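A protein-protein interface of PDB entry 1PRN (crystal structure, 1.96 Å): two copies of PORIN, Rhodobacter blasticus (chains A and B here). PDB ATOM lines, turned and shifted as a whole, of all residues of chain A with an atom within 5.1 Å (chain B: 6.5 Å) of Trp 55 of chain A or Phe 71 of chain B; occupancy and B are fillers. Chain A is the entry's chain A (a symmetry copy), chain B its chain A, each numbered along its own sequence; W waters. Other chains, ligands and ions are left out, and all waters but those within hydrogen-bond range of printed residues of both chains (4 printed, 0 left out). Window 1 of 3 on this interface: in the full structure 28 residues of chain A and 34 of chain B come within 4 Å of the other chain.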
ATOM      1  N   GLY A   8     -23.313 -32.669 -29.407  1.00  0.00           N
ATOM      2  CA  GLY A   8     -22.599 -31.639 -28.692  1.00  0.00           C
ATOM      3  C   GLY A   8     -23.171 -31.698 -27.286  1.00  0.00           C
ATOM      4  O   GLY A   8     -24.291 -32.165 -27.114  1.00  0.00           O
ATOM      5  N   ARG A   9     -22.392 -31.359 -26.272  1.00  0.00           N
ATOM      6  CA  ARG A   9     -22.898 -31.330 -24.910  1.00  0.00           C
ATOM      7  C   ARG A   9     -22.113 -30.281 -24.143  1.00  0.00           C
ATOM      8  O   ARG A   9     -20.958 -29.997 -24.466  1.00  0.00           O
ATOM      9  CB  ARG A   9     -22.813 -32.699 -24.234  1.00  0.00           C
ATOM     10  CG  ARG A   9     -21.473 -33.082 -23.737  1.00  0.00           C
ATOM     11  CD  ARG A   9     -21.536 -34.526 -23.284  1.00  0.00           C
ATOM     12  NE  ARG A   9     -20.261 -34.902 -22.687  1.00  0.00           N
ATOM     13  CZ  ARG A   9     -19.883 -36.142 -22.402  1.00  0.00           C
ATOM     14  NH1 ARG A   9     -20.667 -37.176 -22.657  1.00  0.00           N
ATOM     15  NH2 ARG A   9     -18.721 -36.337 -21.814  1.00  0.00           N
ATOM     16  N   PHE A  10     -22.768 -29.622 -23.201  1.00  0.00           N
ATOM     17  CA  PHE A  10     -22.097 -28.607 -22.400  1.00  0.00           C
ATOM     18  C   PHE A  10     -22.856 -28.409 -21.094  1.00  0.00           C
ATOM     19  O   PHE A  10     -24.046 -28.722 -21.013  1.00  0.00           O
ATOM     20  CB  PHE A  10     -21.917 -27.284 -23.186  1.00  0.00           C
ATOM     21  CG  PHE A  10     -23.207 -26.572 -23.534  1.00  0.00           C
ATOM     22  CD1 PHE A  10     -23.851 -25.767 -22.603  1.00  0.00           C
ATOM     23  CD2 PHE A  10     -23.765 -26.696 -24.799  1.00  0.00           C
ATOM     24  CE1 PHE A  10     -25.023 -25.100 -22.926  1.00  0.00           C
ATOM     25  CE2 PHE A  10     -24.941 -26.025 -25.126  1.00  0.00           C
ATOM     26  CZ  PHE A  10     -25.567 -25.231 -24.188  1.00  0.00           C
ATOM     27  N   SER A  29     -17.327 -29.326 -21.903  1.00  0.00           N
ATOM     28  CA  SER A  29     -18.083 -29.532 -23.120  1.00  0.00           C
ATOM     29  C   SER A  29     -17.379 -30.474 -24.086  1.00  0.00           C
ATOM     30  O   SER A  29     -16.176 -30.707 -23.978  1.00  0.00           O
ATOM     31  CB  SER A  29     -18.367 -28.181 -23.772  1.00  0.00           C
ATOM     32  OG  SER A  29     -17.186 -27.459 -23.988  1.00  0.00           O
ATOM     33  N   ARG A  30     -18.131 -31.018 -25.030  1.00  0.00           N
ATOM     34  CA  ARG A  30     -17.584 -31.951 -26.001  1.00  0.00           C
ATOM     35  C   ARG A  30     -18.314 -31.844 -27.318  1.00  0.00           C
ATOM     36  O   ARG A  30     -19.526 -31.667 -27.354  1.00  0.00           O
ATOM     37  CB  ARG A  30     -17.760 -33.382 -25.477  1.00  0.00           C
ATOM     38  CG  ARG A  30     -17.609 -34.506 -26.535  1.00  0.00           C
ATOM     39  CD  ARG A  30     -17.787 -35.903 -26.046  1.00  0.00           C
ATOM     40  NE  ARG A  30     -16.784 -36.247 -25.048  1.00  0.00           N
ATOM     41  CZ  ARG A  30     -16.708 -37.417 -24.424  1.00  0.00           C
ATOM     42  NH1 ARG A  30     -17.582 -38.383 -24.686  1.00  0.00           N
ATOM     43  NH2 ARG A  30     -15.748 -37.624 -23.535  1.00  0.00           N
ATOM     44  N   LEU A  31     -17.570 -31.896 -28.405  1.00  0.00           N
ATOM     45  CA  LEU A  31     -18.205 -31.902 -29.692  1.00  0.00           C
ATOM     46  C   LEU A  31     -17.716 -33.191 -30.322  1.00  0.00           C
ATOM     47  O   LEU A  31     -16.509 -33.452 -30.328  1.00  0.00           O
ATOM     48  CB  LEU A  31     -17.766 -30.719 -30.536  1.00  0.00           C
ATOM     49  CG  LEU A  31     -18.224 -30.861 -31.995  1.00  0.00           C
ATOM     50  CD1 LEU A  31     -19.743 -30.943 -32.055  1.00  0.00           C
ATOM     51  CD2 LEU A  31     -17.736 -29.696 -32.813  1.00  0.00           C
ATOM     52  N   MET A  53     -13.991 -37.304 -35.098  1.00  0.00           N
ATOM     53  CA  MET A  53     -13.322 -36.057 -34.783  1.00  0.00           C
ATOM     54  C   MET A  53     -14.018 -35.606 -33.502  1.00  0.00           C
ATOM     55  O   MET A  53     -15.209 -35.287 -33.497  1.00  0.00           O
ATOM     56  CB  MET A  53     -13.504 -35.016 -35.881  1.00  0.00           C
ATOM     57  CG  MET A  53     -12.777 -35.349 -37.181  1.00  0.00           C
ATOM     58  SD  MET A  53     -12.890 -33.971 -38.333  1.00  0.00           S
ATOM     59  CE  MET A  53     -11.815 -32.762 -37.476  1.00  0.00           C
ATOM     60  N   GLN A  54     -13.291 -35.646 -32.397  1.00  0.00           N
ATOM     61  CA  GLN A  54     -13.854 -35.259 -31.123  1.00  0.00           C
ATOM     62  C   GLN A  54     -12.988 -34.243 -30.423  1.00  0.00           C
ATOM     63  O   GLN A  54     -11.767 -34.350 -30.430  1.00  0.00           O
ATOM     64  CB  GLN A  54     -14.016 -36.484 -30.244  1.00  0.00           C
ATOM     65  CG  GLN A  54     -14.743 -36.225 -28.927  1.00  0.00           C
ATOM     66  CD  GLN A  54     -14.912 -37.501 -28.144  1.00  0.00           C
ATOM     67  OE1 GLN A  54     -15.531 -38.452 -28.621  1.00  0.00           O
ATOM     68  NE2 GLN A  54     -14.323 -37.555 -26.960  1.00  0.00           N
ATOM     69  N   TRP A  55     -13.635 -33.236 -29.851  1.00  0.00           N
ATOM     70  CA  TRP A  55     -12.954 -32.199 -29.108  1.00  0.00           C
ATOM     71  C   TRP A  55     -13.585 -32.159 -27.730  1.00  0.00           C
ATOM     72  O   TRP A  55     -14.803 -32.306 -27.592  1.00  0.00           O
ATOM     73  CB  TRP A  55     -13.136 -30.829 -29.795  1.00  0.00           C
ATOM     74  CG  TRP A  55     -12.590 -29.667 -28.975  1.00  0.00           C
ATOM     75  CD1 TRP A  55     -11.305 -29.197 -28.976  1.00  0.00           C
ATOM     76  CD2 TRP A  55     -13.287 -28.903 -27.982  1.00  0.00           C
ATOM     77  NE1 TRP A  55     -11.161 -28.213 -28.033  1.00  0.00           N
ATOM     78  CE2 TRP A  55     -12.362 -28.018 -27.403  1.00  0.00           C
ATOM     79  CE3 TRP A  55     -14.615 -28.904 -27.506  1.00  0.00           C
ATOM     80  CZ2 TRP A  55     -12.708 -27.130 -26.390  1.00  0.00           C
ATOM     81  CZ3 TRP A  55     -14.958 -28.028 -26.487  1.00  0.00           C
ATOM     82  CH2 TRP A  55     -14.007 -27.139 -25.945  1.00  0.00           C
ATOM     83  N   ASP A  56     -12.757 -31.985 -26.706  1.00  0.00           N
ATOM     84  CA  ASP A  56     -13.237 -31.849 -25.329  1.00  0.00           C
ATOM     85  C   ASP A  56     -12.549 -30.635 -24.738  1.00  0.00           C
ATOM     86  O   ASP A  56     -11.426 -30.310 -25.131  1.00  0.00           O
ATOM     87  CB  ASP A  56     -12.873 -33.058 -24.483  1.00  0.00           C
ATOM     88  CG  ASP A  56     -13.701 -34.262 -24.804  1.00  0.00           C
ATOM     89  OD1 ASP A  56     -13.310 -35.035 -25.700  1.00  0.00           O
ATOM     90  OD2 ASP A  56     -14.723 -34.462 -24.128  1.00  0.00           O
ATOM     91  N   ASP A  57     -13.206 -29.968 -23.800  1.00  0.00           N
ATOM     92  CA  ASP A  57     -12.610 -28.794 -23.164  1.00  0.00           C
ATOM     93  C   ASP A  57     -11.265 -29.225 -22.555  1.00  0.00           C
ATOM     94  O   ASP A  57     -11.151 -30.324 -22.015  1.00  0.00           O
ATOM     95  CB  ASP A  57     -13.538 -28.224 -22.076  1.00  0.00           C
ATOM     96  CG  ASP A  57     -13.762 -29.190 -20.934  1.00  0.00           C
ATOM     97  OD1 ASP A  57     -14.565 -30.138 -21.070  1.00  0.00           O
ATOM     98  OD2 ASP A  57     -13.111 -29.029 -19.884  1.00  0.00           O
ATOM     99  N   GLY A  58     -10.249 -28.376 -22.653  1.00  0.00           N
ATOM    100  CA  GLY A  58      -8.946 -28.724 -22.111  1.00  0.00           C
ATOM    101  C   GLY A  58      -8.017 -29.444 -23.069  1.00  0.00           C
ATOM    102  O   GLY A  58      -6.846 -29.660 -22.744  1.00  0.00           O
ATOM    103  N   ASP A  59      -8.521 -29.847 -24.236  1.00  0.00           N
ATOM    104  CA  ASP A  59      -7.685 -30.541 -25.217  1.00  0.00           C
ATOM    105  C   ASP A  59      -6.472 -29.704 -25.618  1.00  0.00           C
ATOM    106  O   ASP A  59      -6.571 -28.488 -25.844  1.00  0.00           O
ATOM    107  CB  ASP A  59      -8.474 -30.907 -26.482  1.00  0.00           C
ATOM    108  CG  ASP A  59      -9.224 -32.212 -26.351  1.00  0.00           C
ATOM    109  OD1 ASP A  59      -9.131 -32.870 -25.310  1.00  0.00           O
ATOM    110  OD2 ASP A  59      -9.921 -32.582 -27.309  1.00  0.00           O
ATOM    111  N   ALA A  62      -5.867 -26.562 -28.350  1.00  0.00           N
ATOM    112  CA  ALA A  62      -7.177 -25.976 -28.659  1.00  0.00           C
ATOM    113  C   ALA A  62      -7.581 -26.358 -30.101  1.00  0.00           C
ATOM    114  O   ALA A  62      -8.105 -25.535 -30.862  1.00  0.00           O
ATOM    115  CB  ALA A  62      -7.127 -24.465 -28.475  1.00  0.00           C
ATOM    116  N   GLY A  63      -7.368 -27.627 -30.442  1.00  0.00           N
ATOM    117  CA  GLY A  63      -7.656 -28.130 -31.777  1.00  0.00           C
ATOM    118  C   GLY A  63      -8.326 -29.495 -31.802  1.00  0.00           C
ATOM    119  O   GLY A  63      -8.420 -30.175 -30.784  1.00  0.00           O
ATOM    120  N   THR A  64      -8.745 -29.910 -32.996  1.00  0.00           N
ATOM    121  CA  THR A  64      -9.457 -31.169 -33.197  1.00  0.00           C
ATOM    122  C   THR A  64      -8.882 -31.886 -34.408  1.00  0.00           C
ATOM    123  O   THR A  64      -8.631 -31.273 -35.449  1.00  0.00           O
ATOM    124  CB  THR A  64     -10.975 -30.872 -33.454  1.00  0.00           C
ATOM    125  OG1 THR A  64     -11.459 -30.022 -32.413  1.00  0.00           O
ATOM    126  CG2 THR A  64     -11.819 -32.151 -33.495  1.00  0.00           C
ATOM    127  N   LYS A 120      -9.732 -40.573 -30.065  1.00  0.00           N
ATOM    128  CA  LYS A 120      -8.789 -39.547 -30.482  1.00  0.00           C
ATOM    129  C   LYS A 120      -7.404 -40.102 -30.769  1.00  0.00           C
ATOM    130  O   LYS A 120      -7.136 -41.292 -30.586  1.00  0.00           O
ATOM    131  CB  LYS A 120      -8.651 -38.499 -29.373  1.00  0.00           C
ATOM    132  CG  LYS A 120      -9.931 -37.835 -28.963  1.00  0.00           C
ATOM    133  CD  LYS A 120      -9.548 -36.791 -27.988  1.00  0.00           C
ATOM    134  CE  LYS A 120     -10.867 -36.261 -27.505  1.00  0.00           C
ATOM    135  NZ  LYS A 120     -10.693 -35.120 -26.573  1.00  0.00           N
ATOM    136  N   PHE A 287     -27.246 -32.619 -27.116  1.00  0.00           N
ATOM    137  CA  PHE A 287     -28.124 -32.526 -28.264  1.00  0.00           C
ATOM    138  C   PHE A 287     -27.491 -33.302 -29.421  1.00  0.00           C
ATOM    139  O   PHE A 287     -26.297 -33.177 -29.695  1.00  0.00           O
ATOM    140  CB  PHE A 287     -28.434 -31.070 -28.612  1.00  0.00           C
ATOM    141  CG  PHE A 287     -27.221 -30.205 -28.817  1.00  0.00           C
ATOM    142  CD1 PHE A 287     -26.602 -29.587 -27.738  1.00  0.00           C
ATOM    143  CD2 PHE A 287     -26.734 -29.961 -30.095  1.00  0.00           C
ATOM    144  CE1 PHE A 287     -25.519 -28.731 -27.924  1.00  0.00           C
ATOM    145  CE2 PHE A 287     -25.654 -29.107 -30.285  1.00  0.00           C
ATOM    146  CZ  PHE A 287     -25.050 -28.492 -29.193  1.00  0.00           C
ATOM    147  N   GLY B  48     -26.976 -25.731 -31.466  1.00  0.00           N
ATOM    148  CA  GLY B  48     -26.009 -25.889 -32.523  1.00  0.00           C
ATOM    149  C   GLY B  48     -24.580 -25.948 -32.025  1.00  0.00           C
ATOM    150  O   GLY B  48     -24.281 -25.578 -30.891  1.00  0.00           O
ATOM    151  N   ALA B  49     -23.701 -26.436 -32.882  1.00  0.00           N
ATOM    152  CA  ALA B  49     -22.292 -26.528 -32.566  1.00  0.00           C
ATOM    153  C   ALA B  49     -21.556 -26.317 -33.876  1.00  0.00           C
ATOM    154  O   ALA B  49     -22.098 -26.632 -34.942  1.00  0.00           O
ATOM    155  CB  ALA B  49     -21.966 -27.902 -31.998  1.00  0.00           C
ATOM    156  N   LYS B  50     -20.384 -25.689 -33.829  1.00  0.00           N
ATOM    157  CA  LYS B  50     -19.623 -25.527 -35.044  1.00  0.00           C
ATOM    158  C   LYS B  50     -18.126 -25.721 -34.865  1.00  0.00           C
ATOM    159  O   LYS B  50     -17.574 -25.516 -33.770  1.00  0.00           O
ATOM    160  CB  LYS B  50     -19.941 -24.212 -35.753  1.00  0.00           C
ATOM    161  CG  LYS B  50     -19.374 -23.022 -35.193  1.00  0.00           C
ATOM    162  CD  LYS B  50     -19.161 -22.602 -36.635  1.00  0.00           C
ATOM    163  CE  LYS B  50     -18.262 -21.432 -36.904  1.00  0.00           C
ATOM    164  NZ  LYS B  50     -18.902 -20.149 -36.508  1.00  0.00           N
ATOM    165  N   LEU B  51     -17.499 -26.210 -35.929  1.00  0.00           N
ATOM    166  CA  LEU B  51     -16.066 -26.447 -35.972  1.00  0.00           C
ATOM    167  C   LEU B  51     -15.580 -25.845 -37.287  1.00  0.00           C
ATOM    168  O   LEU B  51     -16.295 -25.858 -38.295  1.00  0.00           O
ATOM    169  CB  LEU B  51     -15.771 -27.958 -35.957  1.00  0.00           C
ATOM    170  CG  LEU B  51     -14.323 -28.410 -35.698  1.00  0.00           C
ATOM    171  CD1 LEU B  51     -14.012 -28.220 -34.239  1.00  0.00           C
ATOM    172  CD2 LEU B  51     -14.127 -29.868 -36.070  1.00  0.00           C
ATOM    173  N   ASN B  67     -10.477 -26.399 -35.219  1.00  0.00           N
ATOM    174  CA  ASN B  67     -10.207 -25.528 -34.084  1.00  0.00           C
ATOM    175  C   ASN B  67     -11.003 -26.024 -32.866  1.00  0.00           C
ATOM    176  O   ASN B  67     -11.397 -27.193 -32.806  1.00  0.00           O
ATOM    177  CB  ASN B  67     -10.572 -24.080 -34.412  1.00  0.00           C
ATOM    178  CG  ASN B  67     -12.030 -23.906 -34.747  1.00  0.00           C
ATOM    179  OD1 ASN B  67     -12.751 -24.884 -34.959  1.00  0.00           O
ATOM    180  ND2 ASN B  67     -12.474 -22.663 -34.829  1.00  0.00           N
ATOM    181  N   ALA B  68     -11.199 -25.159 -31.877  1.00  0.00           N
ATOM    182  CA  ALA B  68     -11.965 -25.528 -30.688  1.00  0.00           C
ATOM    183  C   ALA B  68     -13.443 -25.223 -30.954  1.00  0.00           C
ATOM    184  O   ALA B  68     -13.777 -24.247 -31.640  1.00  0.00           O
ATOM    185  CB  ALA B  68     -11.461 -24.768 -29.485  1.00  0.00           C
ATOM    186  N   ALA B  69     -14.319 -26.050 -30.409  1.00  0.00           N
ATOM    187  CA  ALA B  69     -15.754 -25.915 -30.638  1.00  0.00           C
ATOM    188  C   ALA B  69     -16.471 -24.693 -30.075  1.00  0.00           C
ATOM    189  O   ALA B  69     -16.036 -24.078 -29.097  1.00  0.00           O
ATOM    190  CB  ALA B  69     -16.453 -27.170 -30.149  1.00  0.00           C
ATOM    191  N   GLN B  70     -17.600 -24.372 -30.700  1.00  0.00           N
ATOM    192  CA  GLN B  70     -18.477 -23.296 -30.260  1.00  0.00           C
ATOM    193  C   GLN B  70     -19.858 -23.951 -30.196  1.00  0.00           C
ATOM    194  O   GLN B  70     -20.197 -24.727 -31.092  1.00  0.00           O
ATOM    195  CB  GLN B  70     -18.506 -22.162 -31.274  1.00  0.00           C
ATOM    196  CG  GLN B  70     -19.396 -21.041 -30.850  1.00  0.00           C
ATOM    197  CD  GLN B  70     -19.603 -20.055 -31.963  1.00  0.00           C
ATOM    198  OE1 GLN B  70     -20.627 -20.075 -32.635  1.00  0.00           O
ATOM    199  NE2 GLN B  70     -18.619 -19.210 -32.194  1.00  0.00           N
ATOM    200  N   PHE B  71     -20.625 -23.672 -29.141  1.00  0.00           N
ATOM    201  CA  PHE B  71     -21.962 -24.236 -28.962  1.00  0.00           C
ATOM    202  C   PHE B  71     -22.907 -23.088 -28.740  1.00  0.00           C
ATOM    203  O   PHE B  71     -22.499 -22.055 -28.220  1.00  0.00           O
ATOM    204  CB  PHE B  71     -22.048 -25.122 -27.719  1.00  0.00           C
ATOM    205  CG  PHE B  71     -20.992 -26.186 -27.652  1.00  0.00           C
ATOM    206  CD1 PHE B  71     -19.716 -25.884 -27.162  1.00  0.00           C
ATOM    207  CD2 PHE B  71     -21.254 -27.476 -28.100  1.00  0.00           C
ATOM    208  CE1 PHE B  71     -18.700 -26.848 -27.128  1.00  0.00           C
ATOM    209  CE2 PHE B  71     -20.236 -28.464 -28.071  1.00  0.00           C
ATOM    210  CZ  PHE B  71     -18.956 -28.141 -27.578  1.00  0.00           C
ATOM    211  N   TRP B  72     -24.172 -23.251 -29.104  1.00  0.00           N
ATOM    212  CA  TRP B  72     -25.134 -22.184 -28.868  1.00  0.00           C
ATOM    213  C   TRP B  72     -26.553 -22.695 -28.743  1.00  0.00           C
ATOM    214  O   TRP B  72     -26.865 -23.824 -29.150  1.00  0.00           O
ATOM    215  CB  TRP B  72     -25.072 -21.117 -29.963  1.00  0.00           C
ATOM    216  CG  TRP B  72     -25.562 -21.597 -31.277  1.00  0.00           C
ATOM    217  CD1 TRP B  72     -26.866 -21.653 -31.709  1.00  0.00           C
ATOM    218  CD2 TRP B  72     -24.764 -22.127 -32.339  1.00  0.00           C
ATOM    219  NE1 TRP B  72     -26.920 -22.185 -32.977  1.00  0.00           N
ATOM    220  CE2 TRP B  72     -25.637 -22.476 -33.394  1.00  0.00           C
ATOM    221  CE3 TRP B  72     -23.386 -22.330 -32.508  1.00  0.00           C
ATOM    222  CZ2 TRP B  72     -25.186 -23.027 -34.598  1.00  0.00           C
ATOM    223  CZ3 TRP B  72     -22.931 -22.873 -33.706  1.00  0.00           C
ATOM    224  CH2 TRP B  72     -23.831 -23.216 -34.735  1.00  0.00           C
ATOM    225  N   THR B  73     -27.398 -21.830 -28.191  1.00  0.00           N
ATOM    226  CA  THR B  73     -28.815 -22.079 -27.986  1.00  0.00           C
ATOM    227  C   THR B  73     -29.515 -20.784 -28.370  1.00  0.00           C
ATOM    228  O   THR B  73     -29.166 -19.722 -27.852  1.00  0.00           O
ATOM    229  CB  THR B  73     -29.120 -22.349 -26.503  1.00  0.00           C
ATOM    230  OG1 THR B  73     -28.267 -23.386 -26.026  1.00  0.00           O
ATOM    231  CG2 THR B  73     -30.539 -22.788 -26.335  1.00  0.00           C
ATOM    232  N   VAL B  80     -27.338 -17.685 -26.930  1.00  0.00           N
ATOM    233  CA  VAL B  80     -26.312 -17.806 -25.904  1.00  0.00           C
ATOM    234  C   VAL B  80     -25.287 -18.798 -26.457  1.00  0.00           C
ATOM    235  O   VAL B  80     -25.655 -19.881 -26.900  1.00  0.00           O
ATOM    236  CB  VAL B  80     -26.879 -18.369 -24.600  1.00  0.00           C
ATOM    237  CG1 VAL B  80     -25.788 -18.461 -23.557  1.00  0.00           C
ATOM    238  CG2 VAL B  80     -28.003 -17.492 -24.092  1.00  0.00           C
ATOM    239  N   SER B  81     -24.019 -18.401 -26.516  1.00  0.00           N
ATOM    240  CA  SER B  81     -22.979 -19.286 -27.023  1.00  0.00           C
ATOM    241  C   SER B  81     -21.904 -19.512 -25.974  1.00  0.00           C
ATOM    242  O   SER B  81     -21.711 -18.689 -25.073  1.00  0.00           O
ATOM    243  CB  SER B  81     -22.412 -18.818 -28.374  1.00  0.00           C
ATOM    244  OG  SER B  81     -22.117 -17.470 -28.395  1.00  0.00           O
ATOM    245  N   VAL B  82     -21.260 -20.669 -26.059  1.00  0.00           N
ATOM    246  CA  VAL B  82     -20.242 -21.088 -25.108  1.00  0.00           C
ATOM    247  C   VAL B  82     -19.039 -21.670 -25.856  1.00  0.00           C
ATOM    248  O   VAL B  82     -19.203 -22.251 -26.932  1.00  0.00           O
ATOM    249  CB  VAL B  82     -20.836 -22.211 -24.186  1.00  0.00           C
ATOM    250  CG1 VAL B  82     -19.865 -22.600 -23.098  1.00  0.00           C
ATOM    251  CG2 VAL B  82     -22.128 -21.747 -23.560  1.00  0.00           C
ATOM    252  N   GLY B  83     -17.843 -21.517 -25.284  1.00  0.00           N
ATOM    253  CA  GLY B  83     -16.639 -22.071 -25.882  1.00  0.00           C
ATOM    254  C   GLY B  83     -15.829 -21.047 -26.642  1.00  0.00           C
ATOM    255  O   GLY B  83     -15.419 -20.020 -26.097  1.00  0.00           O
ATOM    256  N   ASN B  84     -15.582 -21.338 -27.909  1.00  0.00           N
ATOM    257  CA  ASN B  84     -14.825 -20.463 -28.791  1.00  0.00           C
ATOM    258  C   ASN B  84     -15.883 -19.532 -29.389  1.00  0.00           C
ATOM    259  O   ASN B  84     -16.399 -19.756 -30.486  1.00  0.00           O
ATOM    260  CB  ASN B  84     -14.159 -21.326 -29.864  1.00  0.00           C
ATOM    261  CG  ASN B  84     -13.245 -20.543 -30.784  1.00  0.00           C
ATOM    262  OD1 ASN B  84     -12.961 -19.341 -30.583  1.00  0.00           O
ATOM    263  ND2 ASN B  84     -12.761 -21.228 -31.808  1.00  0.00           N
ATOM    264  N   VAL B  85     -16.240 -18.515 -28.624  1.00  0.00           N
ATOM    265  CA  VAL B  85     -17.268 -17.567 -29.009  1.00  0.00           C
ATOM    266  C   VAL B  85     -16.816 -16.363 -29.840  1.00  0.00           C
ATOM    267  O   VAL B  85     -15.618 -16.069 -29.973  1.00  0.00           O
ATOM    268  CB  VAL B  85     -18.005 -17.035 -27.738  1.00  0.00           C
ATOM    269  CG1 VAL B  85     -18.588 -18.197 -26.937  1.00  0.00           C
ATOM    270  CG2 VAL B  85     -17.041 -16.225 -26.862  1.00  0.00           C
ATOM    271  N   ASP B 128      -5.539 -23.569 -24.707  1.00  0.00           N
ATOM    272  CA  ASP B 128      -6.008 -24.853 -24.181  1.00  0.00           C
ATOM    273  C   ASP B 128      -7.219 -24.810 -23.247  1.00  0.00           C
ATOM    274  O   ASP B 128      -8.103 -25.643 -23.368  1.00  0.00           O
ATOM    275  CB  ASP B 128      -4.874 -25.630 -23.486  1.00  0.00           C
ATOM    276  CG  ASP B 128      -3.813 -26.144 -24.454  1.00  0.00           C
ATOM    277  OD1 ASP B 128      -3.775 -25.753 -25.643  1.00  0.00           O
ATOM    278  OD2 ASP B 128      -2.982 -26.945 -23.990  1.00  0.00           O
ATOM    279  N   TYR B 130      -9.088 -21.881 -22.680  1.00  0.00           N
ATOM    280  CA  TYR B 130      -9.770 -20.650 -23.029  1.00  0.00           C
ATOM    281  C   TYR B 130     -11.259 -20.970 -23.231  1.00  0.00           C
ATOM    282  O   TYR B 130     -11.619 -21.901 -23.966  1.00  0.00           O
ATOM    283  CB  TYR B 130      -9.125 -20.116 -24.307  1.00  0.00           C
ATOM    284  CG  TYR B 130      -9.803 -18.957 -24.995  1.00  0.00           C
ATOM    285  CD1 TYR B 130     -11.018 -19.126 -25.681  1.00  0.00           C
ATOM    286  CD2 TYR B 130      -9.173 -17.726 -25.071  1.00  0.00           C
ATOM    287  CE1 TYR B 130     -11.566 -18.095 -26.434  1.00  0.00           C
ATOM    288  CE2 TYR B 130      -9.708 -16.685 -25.827  1.00  0.00           C
ATOM    289  CZ  TYR B 130     -10.898 -16.874 -26.514  1.00  0.00           C
ATOM    290  OH  TYR B 130     -11.364 -15.868 -27.329  1.00  0.00           O
ATOM    291  N   ASN B 131     -12.125 -20.216 -22.568  1.00  0.00           N
ATOM    292  CA  ASN B 131     -13.556 -20.440 -22.676  1.00  0.00           C
ATOM    293  C   ASN B 131     -14.313 -19.122 -22.539  1.00  0.00           C
ATOM    294  O   ASN B 131     -14.009 -18.327 -21.653  1.00  0.00           O
ATOM    295  CB  ASN B 131     -14.001 -21.408 -21.588  1.00  0.00           C
ATOM    296  CG  ASN B 131     -15.381 -21.974 -21.839  1.00  0.00           C
ATOM    297  OD1 ASN B 131     -15.547 -22.847 -22.683  1.00  0.00           O
ATOM    298  ND2 ASN B 131     -16.372 -21.479 -21.120  1.00  0.00           N
HETATM  299  O   HOH W   1      -9.107 -23.014 -31.390  1.00  0.00           O
HETATM  300  O   HOH W   2     -16.207 -25.683 -22.475  1.00  0.00           O
HETATM  301  O   HOH W   3     -11.091 -25.742 -23.318  1.00  0.00           O
HETATM  302  O   HOH W   4      -8.948 -27.220 -26.348  1.00  0.00           O
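O of Asn 67 of chain B lies within hydrogen-bond range of OG1 of Thr 64 of chain A (2.9 Å).
N of Ala 68 of chain B lies within hydrogen-bond range of O of Ala 62 of chain A, 3.3 Å away.
Hydrophobic or aromatic side chains of chain B that line the printed part of chain A: Ala 49, Leu 51, Ala 68, Ala 69 and Phe 71.
Hydrophobic or aromatic side chains of chain A within 4 Å of the printed part of chain B: Phe 10, Leu 31, Met 53, Trp 55 and Phe 287.
Water W2 lies within hydrogen-bond range of OG of Ser 29 of chain A (2.5 Å) and OD1 of Asn 131 of chain B (2.9 Å).
Water W4 lies within hydrogen-bond range of O of Asp 59 of chain A (2.7 Å), NE1 of Trp 55 of chain A (3.0 Å) and O of Asp 128 of chain B (3.5 Å).
Water W1 lies within hydrogen-bond range of O of Ala 62 of chain A and N of Ala 68 of chain B.
Water W3 lies within hydrogen-bond range of the backbone NH (N) of Gly 58 of chain A and the backbone carbonyl oxygen (O) of Asp 128 of chain B.
The side-chain amide nitrogen (ND2) of Asn 84 of chain B lies within hydrogen-bond range of the backbone carbonyl oxygen (O) of Ala 68 of chain B (3.2 Å).
The side-chain carboxylate (OD2) of Asp 59 of chain A is in salt-bridge range of the side-chain amino group (NZ) of Lys 120 of chain A.
The backbone NH (N) of Leu 31 of chain A sits at hydrogen-bond distance from the backbone carbonyl oxygen (O) of Trp 55 of chain A (2.9 Å).
ND2 of Asn 67 of chain B sits close to ND2 of Asn 84 of chain B (3.4 Å).
The backbone carbonyl oxygen (O) of Arg 9 of chain A lies within hydrogen-bond range of the backbone NH (N) of Arg 30 of chain A (3.1 Å).
N of Asp 56 of chain A sits at hydrogen-bond distance from OD2 of Asp 59 of chain A (3.0 Å).
Arg 9 of chain A touches Phe 71 of chain B (O to CE2, 3.98 Å).
Ser 29 of chain A touches Phe 71 of chain B (OG to CE1, 3.5 Å).
Met 53 of chain A touches Leu 51 of chain B (CE to CD2, 3.96 Å).
NE1 of Trp 55 of chain A touches CB of Ala 68 of chain B (3.8 Å).
CB of Ala 69 of chain B touches CE3 of Trp 55 of chain A, at 3.7 Å.
Phe 71 of chain B touches Trp 55 of chain A.
O of Asp 128 of chain B touches CA of Gly 58 of chain A (3.4 Å).
Asp 128 of chain B touches Asp 59 of chain A.
Thr 64 of chain A touches Leu 51 of chain B (OG1 to CD1, 3.6 Å).
CZ of Phe 287 of chain A touches O of Gly 48 of chain B, 3.5 Å away.
Of the printed residues of chain B, Phe 10 of chain A touches Phe 71 and Thr 73.
Printed residues of chain B within 4 Å of Arg 30 of chain A: Phe 71 (3.4 Å).
Gln 54 of chain A touches none of the printed residues of chain B.
Trp 55 of chain A touches just these residues of chain B: Ala 68, Ala 69 and Phe 71.
Asp 56 of chain A touches none of the printed residues of chain B.
Of the printed residues of chain B, Thr 64 of chain A touches Leu 51 and Asn 67.
Of the printed residues of chain B, Phe 287 of chain A touches Gly 48.
Of the printed residues of chain A, Leu 51 of chain B touches Met 53 (3.96 Å) and Thr 64 (3.6 Å).
Of the printed residues of chain A, Phe 71 of chain B touches Arg 9, Phe 10, Ser 29, Arg 30 and Trp 55.
The nearest printed residue of chain B that does not touch Thr 64 of chain A is Ala 68 of chain B (4.8 Å).
No position is printed for both chains.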
